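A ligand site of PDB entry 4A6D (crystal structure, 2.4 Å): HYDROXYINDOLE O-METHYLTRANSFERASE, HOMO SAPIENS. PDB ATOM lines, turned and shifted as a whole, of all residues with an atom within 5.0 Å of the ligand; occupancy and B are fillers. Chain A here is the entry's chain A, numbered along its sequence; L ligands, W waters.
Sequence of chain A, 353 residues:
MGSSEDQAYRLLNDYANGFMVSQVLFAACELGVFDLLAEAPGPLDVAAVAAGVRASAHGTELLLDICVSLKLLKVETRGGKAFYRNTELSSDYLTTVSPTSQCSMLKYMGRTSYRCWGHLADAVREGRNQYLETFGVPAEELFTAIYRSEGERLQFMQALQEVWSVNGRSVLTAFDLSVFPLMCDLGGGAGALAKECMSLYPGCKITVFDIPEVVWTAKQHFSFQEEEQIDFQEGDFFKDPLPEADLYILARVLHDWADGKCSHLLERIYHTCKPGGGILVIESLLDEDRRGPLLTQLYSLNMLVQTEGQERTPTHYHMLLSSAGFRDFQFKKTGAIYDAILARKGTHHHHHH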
ATOM      1  N   PHE A 143      11.930 -11.136   6.155  1.00  0.00           N
ATOM      2  CA  PHE A 143      12.152 -12.105   7.215  1.00  0.00           C
ATOM      3  C   PHE A 143      11.943 -13.617   6.876  1.00  0.00           C
ATOM      4  O   PHE A 143      12.550 -14.456   7.544  1.00  0.00           O
ATOM      5  CB  PHE A 143      11.583 -11.641   8.575  1.00  0.00           C
ATOM      6  CG  PHE A 143      12.484 -10.602   9.225  1.00  0.00           C
ATOM      7  CD1 PHE A 143      13.574 -10.986   9.988  1.00  0.00           C
ATOM      8  CD2 PHE A 143      12.277  -9.239   8.995  1.00  0.00           C
ATOM      9  CE1 PHE A 143      14.410 -10.031  10.581  1.00  0.00           C
ATOM     10  CE2 PHE A 143      13.129  -8.290   9.577  1.00  0.00           C
ATOM     11  CZ  PHE A 143      14.186  -8.692  10.359  1.00  0.00           C
ATOM     12  N   TYR A 147      14.770 -15.966   7.998  1.00  0.00           N
ATOM     13  CA  TYR A 147      14.442 -17.186   8.751  1.00  0.00           C
ATOM     14  C   TYR A 147      14.062 -18.327   7.771  1.00  0.00           C
ATOM     15  O   TYR A 147      12.978 -18.902   7.850  1.00  0.00           O
ATOM     16  CB  TYR A 147      13.312 -16.957   9.778  1.00  0.00           C
ATOM     17  CG  TYR A 147      13.423 -15.719  10.643  1.00  0.00           C
ATOM     18  CD1 TYR A 147      14.615 -15.383  11.284  1.00  0.00           C
ATOM     19  CD2 TYR A 147      12.303 -14.927  10.909  1.00  0.00           C
ATOM     20  CE1 TYR A 147      14.707 -14.270  12.112  1.00  0.00           C
ATOM     21  CE2 TYR A 147      12.392 -13.799  11.724  1.00  0.00           C
ATOM     22  CZ  TYR A 147      13.589 -13.482  12.344  1.00  0.00           C
ATOM     23  OH  TYR A 147      13.683 -12.379  13.161  1.00  0.00           O
ATOM     24  N   PHE A 156      19.918 -16.779  14.192  1.00  0.00           N
ATOM     25  CA  PHE A 156      19.716 -15.327  14.038  1.00  0.00           C
ATOM     26  C   PHE A 156      19.383 -14.695  15.401  1.00  0.00           C
ATOM     27  O   PHE A 156      20.005 -13.712  15.809  1.00  0.00           O
ATOM     28  CB  PHE A 156      18.588 -15.027  13.021  1.00  0.00           C
ATOM     29  CG  PHE A 156      18.364 -13.560  12.742  1.00  0.00           C
ATOM     30  CD1 PHE A 156      19.148 -12.873  11.827  1.00  0.00           C
ATOM     31  CD2 PHE A 156      17.364 -12.852  13.433  1.00  0.00           C
ATOM     32  CE1 PHE A 156      18.954 -11.507  11.597  1.00  0.00           C
ATOM     33  CE2 PHE A 156      17.168 -11.478  13.197  1.00  0.00           C
ATOM     34  CZ  PHE A 156      17.951 -10.813  12.273  1.00  0.00           C
ATOM     35  N   LEU A 160      21.655 -11.973  17.523  1.00  0.00           N
ATOM     36  CA  LEU A 160      21.185 -10.631  17.858  1.00  0.00           C
ATOM     37  C   LEU A 160      21.126 -10.238  19.331  1.00  0.00           C
ATOM     38  O   LEU A 160      21.388  -9.085  19.650  1.00  0.00           O
ATOM     39  CB  LEU A 160      19.927 -10.239  17.055  1.00  0.00           C
ATOM     40  CG  LEU A 160      20.258  -9.650  15.661  1.00  0.00           C
ATOM     41  CD1 LEU A 160      20.692 -10.723  14.665  1.00  0.00           C
ATOM     42  CD2 LEU A 160      19.137  -8.861  15.105  1.00  0.00           C
ATOM     43  N   GLN A 161      20.872 -11.210  20.237  1.00  0.00           N
ATOM     44  CA  GLN A 161      20.794 -10.941  21.673  1.00  0.00           C
ATOM     45  C   GLN A 161      22.117 -10.518  22.315  1.00  0.00           C
ATOM     46  O   GLN A 161      22.142  -9.802  23.331  1.00  0.00           O
ATOM     47  CB  GLN A 161      20.141 -12.116  22.431  1.00  0.00           C
ATOM     48  CG  GLN A 161      21.042 -13.318  22.754  1.00  0.00           C
ATOM     49  CD  GLN A 161      20.342 -14.341  23.607  1.00  0.00           C
ATOM     50  OE1 GLN A 161      19.193 -14.156  24.067  1.00  0.00           O
ATOM     51  NE2 GLN A 161      21.040 -15.453  23.866  1.00  0.00           N
ATOM     52  N   TRP A 164      23.403  -6.732  23.275  1.00  0.00           N
ATOM     53  CA  TRP A 164      22.789  -6.156  24.455  1.00  0.00           C
ATOM     54  C   TRP A 164      23.486  -6.478  25.783  1.00  0.00           C
ATOM     55  O   TRP A 164      23.365  -5.695  26.742  1.00  0.00           O
ATOM     56  CB  TRP A 164      21.272  -6.353  24.443  1.00  0.00           C
ATOM     57  CG  TRP A 164      20.659  -5.990  23.108  1.00  0.00           C
ATOM     58  CD1 TRP A 164      19.918  -6.804  22.304  1.00  0.00           C
ATOM     59  CD2 TRP A 164      20.821  -4.748  22.389  1.00  0.00           C
ATOM     60  NE1 TRP A 164      19.613  -6.166  21.125  1.00  0.00           N
ATOM     61  CE2 TRP A 164      20.141  -4.886  21.162  1.00  0.00           C
ATOM     62  CE3 TRP A 164      21.523  -3.545  22.656  1.00  0.00           C
ATOM     63  CZ2 TRP A 164      20.100  -3.863  20.205  1.00  0.00           C
ATOM     64  CZ3 TRP A 164      21.484  -2.529  21.705  1.00  0.00           C
ATOM     65  CH2 TRP A 164      20.781  -2.696  20.498  1.00  0.00           C
ATOM     66  N   ASP A 185       8.447  -3.836  23.489  1.00  0.00           N
ATOM     67  CA  ASP A 185       9.605  -3.983  22.599  1.00  0.00           C
ATOM     68  C   ASP A 185       9.101  -4.562  21.282  1.00  0.00           C
ATOM     69  O   ASP A 185       8.801  -5.758  21.206  1.00  0.00           O
ATOM     70  CB  ASP A 185      10.724  -4.854  23.201  1.00  0.00           C
ATOM     71  CG  ASP A 185      12.067  -4.709  22.498  1.00  0.00           C
ATOM     72  OD1 ASP A 185      12.131  -3.959  21.494  1.00  0.00           O
ATOM     73  OD2 ASP A 185      13.041  -5.363  22.935  1.00  0.00           O
ATOM     74  N   GLY A 187       9.359  -5.967  17.893  1.00  0.00           N
ATOM     75  CA  GLY A 187      10.398  -6.711  17.185  1.00  0.00           C
ATOM     76  C   GLY A 187      11.466  -7.061  18.194  1.00  0.00           C
ATOM     77  O   GLY A 187      12.648  -7.009  17.885  1.00  0.00           O
ATOM     78  N   GLY A 188      11.033  -7.342  19.419  1.00  0.00           N
ATOM     79  CA  GLY A 188      11.908  -7.628  20.555  1.00  0.00           C
ATOM     80  C   GLY A 188      12.711  -8.901  20.520  1.00  0.00           C
ATOM     81  O   GLY A 188      13.564  -9.106  21.393  1.00  0.00           O
ATOM     82  N   GLY A 189      12.420  -9.786  19.552  1.00  0.00           N
ATOM     83  CA  GLY A 189      13.116 -11.052  19.360  1.00  0.00           C
ATOM     84  C   GLY A 189      13.028 -11.988  20.555  1.00  0.00           C
ATOM     85  O   GLY A 189      11.941 -12.237  21.076  1.00  0.00           O
ATOM     86  N   PHE A 209       7.007  -7.935  21.524  1.00  0.00           N
ATOM     87  CA  PHE A 209       6.177  -8.151  20.339  1.00  0.00           C
ATOM     88  C   PHE A 209       7.027  -8.619  19.159  1.00  0.00           C
ATOM     89  O   PHE A 209       8.018  -7.996  18.801  1.00  0.00           O
ATOM     90  CB  PHE A 209       5.384  -6.882  19.973  1.00  0.00           C
ATOM     91  CG  PHE A 209       4.338  -7.086  18.909  1.00  0.00           C
ATOM     92  CD1 PHE A 209       4.674  -7.051  17.553  1.00  0.00           C
ATOM     93  CD2 PHE A 209       3.007  -7.336  19.252  1.00  0.00           C
ATOM     94  CE1 PHE A 209       3.695  -7.244  16.573  1.00  0.00           C
ATOM     95  CE2 PHE A 209       2.038  -7.509  18.276  1.00  0.00           C
ATOM     96  CZ  PHE A 209       2.384  -7.458  16.948  1.00  0.00           C
ATOM     97  N   ASP A 210       6.621  -9.720  18.534  1.00  0.00           N
ATOM     98  CA  ASP A 210       7.331 -10.270  17.373  1.00  0.00           C
ATOM     99  C   ASP A 210       6.434 -11.227  16.603  1.00  0.00           C
ATOM    100  O   ASP A 210       5.307 -11.483  17.023  1.00  0.00           O
ATOM    101  CB  ASP A 210       8.680 -10.906  17.770  1.00  0.00           C
ATOM    102  CG  ASP A 210       9.792 -10.622  16.769  1.00  0.00           C
ATOM    103  OD1 ASP A 210       9.685 -11.114  15.626  1.00  0.00           O
ATOM    104  OD2 ASP A 210      10.799  -9.957  17.152  1.00  0.00           O
ATOM    105  N   ILE A 211       6.934 -11.728  15.454  1.00  0.00           N
ATOM    106  CA  ILE A 211       6.197 -12.646  14.600  1.00  0.00           C
ATOM    107  C   ILE A 211       6.024 -13.989  15.319  1.00  0.00           C
ATOM    108  O   ILE A 211       6.956 -14.382  16.052  1.00  0.00           O
ATOM    109  CB  ILE A 211       6.846 -12.778  13.172  1.00  0.00           C
ATOM    110  CG1 ILE A 211       8.223 -13.462  13.221  1.00  0.00           C
ATOM    111  CG2 ILE A 211       6.894 -11.428  12.445  1.00  0.00           C
ATOM    112  CD1 ILE A 211       8.680 -14.099  11.941  1.00  0.00           C
ATOM    113  N   VAL A 214       9.026 -16.351  15.934  1.00  0.00           N
ATOM    114  CA  VAL A 214      10.061 -15.850  16.841  1.00  0.00           C
ATOM    115  C   VAL A 214       9.616 -16.042  18.293  1.00  0.00           C
ATOM    116  O   VAL A 214      10.374 -16.561  19.097  1.00  0.00           O
ATOM    117  CB  VAL A 214      10.496 -14.393  16.501  1.00  0.00           C
ATOM    118  CG1 VAL A 214      11.327 -13.762  17.619  1.00  0.00           C
ATOM    119  CG2 VAL A 214      11.251 -14.344  15.178  1.00  0.00           C
ATOM    120  N   GLY A 235       2.490 -11.426  16.643  1.00  0.00           N
ATOM    121  CA  GLY A 235       1.771 -10.748  15.587  1.00  0.00           C
ATOM    122  C   GLY A 235       2.632 -10.036  14.563  1.00  0.00           C
ATOM    123  O   GLY A 235       3.865 -10.214  14.515  1.00  0.00           O
ATOM    124  N   ASP A 236       1.978  -9.225  13.733  1.00  0.00           N
ATOM    125  CA  ASP A 236       2.615  -8.433  12.697  1.00  0.00           C
ATOM    126  C   ASP A 236       2.457  -6.939  13.030  1.00  0.00           C
ATOM    127  O   ASP A 236       1.355  -6.422  12.948  1.00  0.00           O
ATOM    128  CB  ASP A 236       2.015  -8.792  11.311  1.00  0.00           C
ATOM    129  CG  ASP A 236       2.492  -7.930  10.152  1.00  0.00           C
ATOM    130  OD1 ASP A 236       3.470  -7.129  10.347  1.00  0.00           O
ATOM    131  OD2 ASP A 236       1.932  -8.067   9.060  1.00  0.00           O
ATOM    132  N   PHE A 237       3.554  -6.249  13.345  1.00  0.00           N
ATOM    133  CA  PHE A 237       3.434  -4.823  13.701  1.00  0.00           C
ATOM    134  C   PHE A 237       2.931  -3.863  12.609  1.00  0.00           C
ATOM    135  O   PHE A 237       2.495  -2.743  12.911  1.00  0.00           O
ATOM    136  CB  PHE A 237       4.616  -4.287  14.507  1.00  0.00           C
ATOM    137  CG  PHE A 237       6.008  -4.472  13.961  1.00  0.00           C
ATOM    138  CD1 PHE A 237       6.276  -4.277  12.598  1.00  0.00           C
ATOM    139  CD2 PHE A 237       7.072  -4.758  14.804  1.00  0.00           C
ATOM    140  CE1 PHE A 237       7.576  -4.362  12.104  1.00  0.00           C
ATOM    141  CE2 PHE A 237       8.369  -4.889  14.293  1.00  0.00           C
ATOM    142  CZ  PHE A 237       8.604  -4.711  12.947  1.00  0.00           C
ATOM    143  N   PHE A 238       2.868  -4.344  11.350  1.00  0.00           N
ATOM    144  CA  PHE A 238       2.348  -3.576  10.224  1.00  0.00           C
ATOM    145  C   PHE A 238       0.852  -3.614  10.111  1.00  0.00           C
ATOM    146  O   PHE A 238       0.291  -2.779   9.399  1.00  0.00           O
ATOM    147  CB  PHE A 238       2.993  -3.995   8.880  1.00  0.00           C
ATOM    148  CG  PHE A 238       4.431  -3.557   8.780  1.00  0.00           C
ATOM    149  CD1 PHE A 238       4.763  -2.211   8.757  1.00  0.00           C
ATOM    150  CD2 PHE A 238       5.451  -4.494   8.738  1.00  0.00           C
ATOM    151  CE1 PHE A 238       6.106  -1.806   8.704  1.00  0.00           C
ATOM    152  CE2 PHE A 238       6.789  -4.093   8.637  1.00  0.00           C
ATOM    153  CZ  PHE A 238       7.104  -2.744   8.666  1.00  0.00           C
ATOM    154  N   ALA A 251      14.348  -1.298  18.513  1.00  0.00           N
ATOM    155  CA  ALA A 251      15.816  -1.545  18.469  1.00  0.00           C
ATOM    156  C   ALA A 251      16.116  -2.376  17.230  1.00  0.00           C
ATOM    157  O   ALA A 251      15.594  -3.492  17.083  1.00  0.00           O
ATOM    158  CB  ALA A 251      16.278  -2.265  19.731  1.00  0.00           C
ATOM    159  N   ARG A 252      16.895  -1.785  16.304  1.00  0.00           N
ATOM    160  CA  ARG A 252      17.294  -2.396  15.035  1.00  0.00           C
ATOM    161  C   ARG A 252      16.096  -2.863  14.201  1.00  0.00           C
ATOM    162  O   ARG A 252      16.126  -3.929  13.584  1.00  0.00           O
ATOM    163  CB  ARG A 252      18.332  -3.519  15.233  1.00  0.00           C
ATOM    164  CG  ARG A 252      19.700  -3.025  15.706  1.00  0.00           C
ATOM    165  CD  ARG A 252      20.159  -3.957  16.791  1.00  0.00           C
ATOM    166  NE  ARG A 252      21.313  -4.754  16.382  1.00  0.00           N
ATOM    167  CZ  ARG A 252      21.670  -5.901  16.948  1.00  0.00           C
ATOM    168  NH1 ARG A 252      20.923  -6.446  17.899  1.00  0.00           N
ATOM    169  NH2 ARG A 252      22.772  -6.517  16.547  1.00  0.00           N
ATOM    170  N   VAL A 253      15.032  -2.067  14.196  1.00  0.00           N
ATOM    171  CA  VAL A 253      13.875  -2.409  13.395  1.00  0.00           C
ATOM    172  C   VAL A 253      13.895  -1.460  12.199  1.00  0.00           C
ATOM    173  O   VAL A 253      13.919  -1.927  11.095  1.00  0.00           O
ATOM    174  CB  VAL A 253      12.551  -2.345  14.223  1.00  0.00           C
ATOM    175  CG1 VAL A 253      11.335  -2.409  13.300  1.00  0.00           C
ATOM    176  CG2 VAL A 253      12.512  -3.438  15.272  1.00  0.00           C
ATOM    177  N   HIS A 255      16.178   0.325  10.688  1.00  0.00           N
ATOM    178  CA  HIS A 255      17.263   0.153   9.716  1.00  0.00           C
ATOM    179  C   HIS A 255      17.016  -0.961   8.675  1.00  0.00           C
ATOM    180  O   HIS A 255      17.686  -0.951   7.638  1.00  0.00           O
ATOM    181  CB  HIS A 255      18.632   0.058  10.422  1.00  0.00           C
ATOM    182  CG  HIS A 255      18.926  -1.280  11.038  1.00  0.00           C
ATOM    183  ND1 HIS A 255      20.222  -1.685  11.309  1.00  0.00           N
ATOM    184  CD2 HIS A 255      18.085  -2.273  11.401  1.00  0.00           C
ATOM    185  CE1 HIS A 255      20.119  -2.910  11.813  1.00  0.00           C
ATOM    186  NE2 HIS A 255      18.856  -3.290  11.903  1.00  0.00           N
ATOM    187  N   ASP A 256      16.043  -1.883   8.922  1.00  0.00           N
ATOM    188  CA  ASP A 256      15.756  -2.994   7.995  1.00  0.00           C
ATOM    189  C   ASP A 256      14.914  -2.569   6.808  1.00  0.00           C
ATOM    190  O   ASP A 256      14.794  -3.319   5.838  1.00  0.00           O
ATOM    191  CB  ASP A 256      14.984  -4.123   8.712  1.00  0.00           C
ATOM    192  CG  ASP A 256      15.663  -4.829   9.879  1.00  0.00           C
ATOM    193  OD1 ASP A 256      16.910  -5.036   9.812  1.00  0.00           O
ATOM    194  OD2 ASP A 256      14.936  -5.280  10.807  1.00  0.00           O
ATOM    195  N   TRP A 257      14.279  -1.396   6.918  1.00  0.00           N
ATOM    196  CA  TRP A 257      13.308  -0.938   5.941  1.00  0.00           C
ATOM    197  C   TRP A 257      13.569   0.417   5.359  1.00  0.00           C
ATOM    198  O   TRP A 257      14.213   1.262   5.985  1.00  0.00           O
ATOM    199  CB  TRP A 257      11.902  -0.914   6.600  1.00  0.00           C
ATOM    200  CG  TRP A 257      11.555  -2.100   7.464  1.00  0.00           C
ATOM    201  CD1 TRP A 257      11.425  -2.114   8.824  1.00  0.00           C
ATOM    202  CD2 TRP A 257      11.237  -3.422   7.013  1.00  0.00           C
ATOM    203  NE1 TRP A 257      11.032  -3.366   9.251  1.00  0.00           N
ATOM    204  CE2 TRP A 257      10.935  -4.196   8.164  1.00  0.00           C
ATOM    205  CE3 TRP A 257      11.133  -4.033   5.745  1.00  0.00           C
ATOM    206  CZ2 TRP A 257      10.548  -5.545   8.079  1.00  0.00           C
ATOM    207  CZ3 TRP A 257      10.728  -5.362   5.657  1.00  0.00           C
ATOM    208  CH2 TRP A 257      10.440  -6.109   6.817  1.00  0.00           C
HETATM  209  N1  LIG L   1      15.090  -5.809  18.547  1.00  0.00           N
HETATM  210  C1  LIG L   1      15.999  -6.974  18.440  1.00  0.00           C
HETATM  211  C2  LIG L   1      17.502  -6.705  18.646  1.00  0.00           C
HETATM  212  O1  LIG L   1      17.927  -5.601  18.380  1.00  0.00           O
HETATM  213  O2  LIG L   1      18.314  -7.587  19.075  1.00  0.00           O
HETATM  214  C3  LIG L   1      15.692  -7.642  17.117  1.00  0.00           C
HETATM  215  C4  LIG L   1      16.130  -6.820  15.897  1.00  0.00           C
HETATM  216  S1  LIG L   1      15.792  -7.818  14.399  1.00  0.00           S
HETATM  217  C5  LIG L   1      16.771  -6.979  13.230  1.00  0.00           C
HETATM  218  C6  LIG L   1      14.198  -7.176  13.801  1.00  0.00           C
HETATM  219  C7  LIG L   1      13.120  -7.931  14.597  1.00  0.00           C
HETATM  220  O3  LIG L   1      11.895  -7.491  14.040  1.00  0.00           O
HETATM  221  C8  LIG L   1      13.204  -9.491  14.403  1.00  0.00           C
HETATM  222  O4  LIG L   1      13.176 -10.177  15.669  1.00  0.00           O
HETATM  223  C9  LIG L   1      11.977  -9.775  13.474  1.00  0.00           C
HETATM  224  O5  LIG L   1      11.342 -11.051  13.581  1.00  0.00           O
HETATM  225  C10 LIG L   1      11.026  -8.649  13.916  1.00  0.00           C
HETATM  226  N2  LIG L   1       9.980  -8.359  12.898  1.00  0.00           N
HETATM  227  C11 LIG L   1      10.175  -8.194  11.535  1.00  0.00           C
HETATM  228  N3  LIG L   1       9.048  -7.941  10.949  1.00  0.00           N
HETATM  229  C12 LIG L   1       8.024  -7.983  11.889  1.00  0.00           C
HETATM  230  C13 LIG L   1       6.627  -7.816  11.877  1.00  0.00           C
HETATM  231  N4  LIG L   1       6.020  -7.487  10.710  1.00  0.00           N
HETATM  232  N5  LIG L   1       5.912  -7.892  13.060  1.00  0.00           N
HETATM  233  C14 LIG L   1       6.512  -8.221  14.215  1.00  0.00           C
HETATM  234  N6  LIG L   1       7.850  -8.390  14.253  1.00  0.00           N
HETATM  235  C15 LIG L   1       8.631  -8.233  13.168  1.00  0.00           C
HETATM  236  O   HOH W   1      12.907  -3.529  18.957  1.00  0.00           O
HETATM  237  O   HOH W   2      15.493  -6.424  21.495  1.00  0.00           O
HETATM  238  O   HOH W   3      12.381  -5.440  11.485  1.00  0.00           O
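The side-chain carboxylate (OD1) of Asp 236 is in hydrogen-bond range of a nitrogen (N4) of the ligand, at 2.6 Å.
OD1 of Asp 210 sits at hydrogen-bond distance from O5 of the ligand, at 2.6 Å.
An oxygen (O5) of the ligand lies within hydrogen-bond range of the side-chain hydroxyl of Tyr 147, at 2.7 Å.
N1 of the ligand lies within hydrogen-bond range of O of Ala 251 (2.8 Å).
N1 of the ligand lies within hydrogen-bond range of O of Gly 187, 2.8 Å away.
The indole nitrogen (NE1) of Trp 164 lies within hydrogen-bond range of an oxygen (O2) of the ligand (2.8 Å).
A nitrogen (N5) of the ligand is in hydrogen-bond range of the backbone NH of Phe 237, at 2.9 Å.
NH1 of Arg 252 is in salt-bridge range of O2 of the ligand (3.1 Å).
N of Phe 238 sits at hydrogen-bond distance from OD1 of Asp 236 (3.0 Å).
N of Gly 189 lies within hydrogen-bond range of OD2 of Asp 210 (2.9 Å).
N of Gly 188 lies within hydrogen-bond range of OD2 of Asp 210 (3.5 Å).
NH1 of Arg 252 sits at hydrogen-bond distance from O of Leu 160 (3.2 Å).
O of Arg 252 sits at hydrogen-bond distance from NE2 of His 255, 3.3 Å away.
OD1 of Asp 256 sits at hydrogen-bond distance from NE2 of His 255, 3.3 Å away.
O of Phe 209 is in hydrogen-bond range of N of Gly 188, 3.1 Å away.
The backbone NH of Phe 209 sits at hydrogen-bond distance from the backbone carbonyl oxygen of Asp 185 (2.8 Å).
An oxygen (O2) of the ligand sits close to the backbone carbonyl oxygen (O) of Leu 160 (3.5 Å).
O of Gly 235 lies close to N5 of the ligand (3.4 Å).
Residues that only touch the ligand: Phe 143 (3.5 Å), Gly 189 (3.8 Å), Phe 209 (3.8 Å), Ile 211 (3.7 Å), Val 214 (3.7 Å), Phe 238 (3.6 Å) and Asp 256 (3.5 Å).
17 residues have an atom within 4 Å of the ligand: Phe 143, Tyr 147, Leu 160, Trp 164, Gly 187, Gly 189, Phe 209, Asp 210, Ile 211, Val 214, Gly 235, Asp 236, Phe 237, Phe 238, Ala 251, Arg 252 and Asp 256.
The nearest printed residue that does not touch the ligand is Trp 257 (4.03 Å).
Water W2 lies within hydrogen-bond range of the side-chain carboxylate (OD2) of Asp 185, a nitrogen (N1) of the ligand and the backbone carbonyl oxygen (O) of Gly 188.
Water W1 lies within hydrogen-bond range of OD1 of Asp 185 (2.7 Å), N of Ala 251 (2.7 Å) and N1 of the ligand (3.2 Å).
Water W3 lies within hydrogen-bond range of the side-chain carboxylate of Asp 256, an oxygen (O3) of the ligand and the indole nitrogen of Trp 257.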
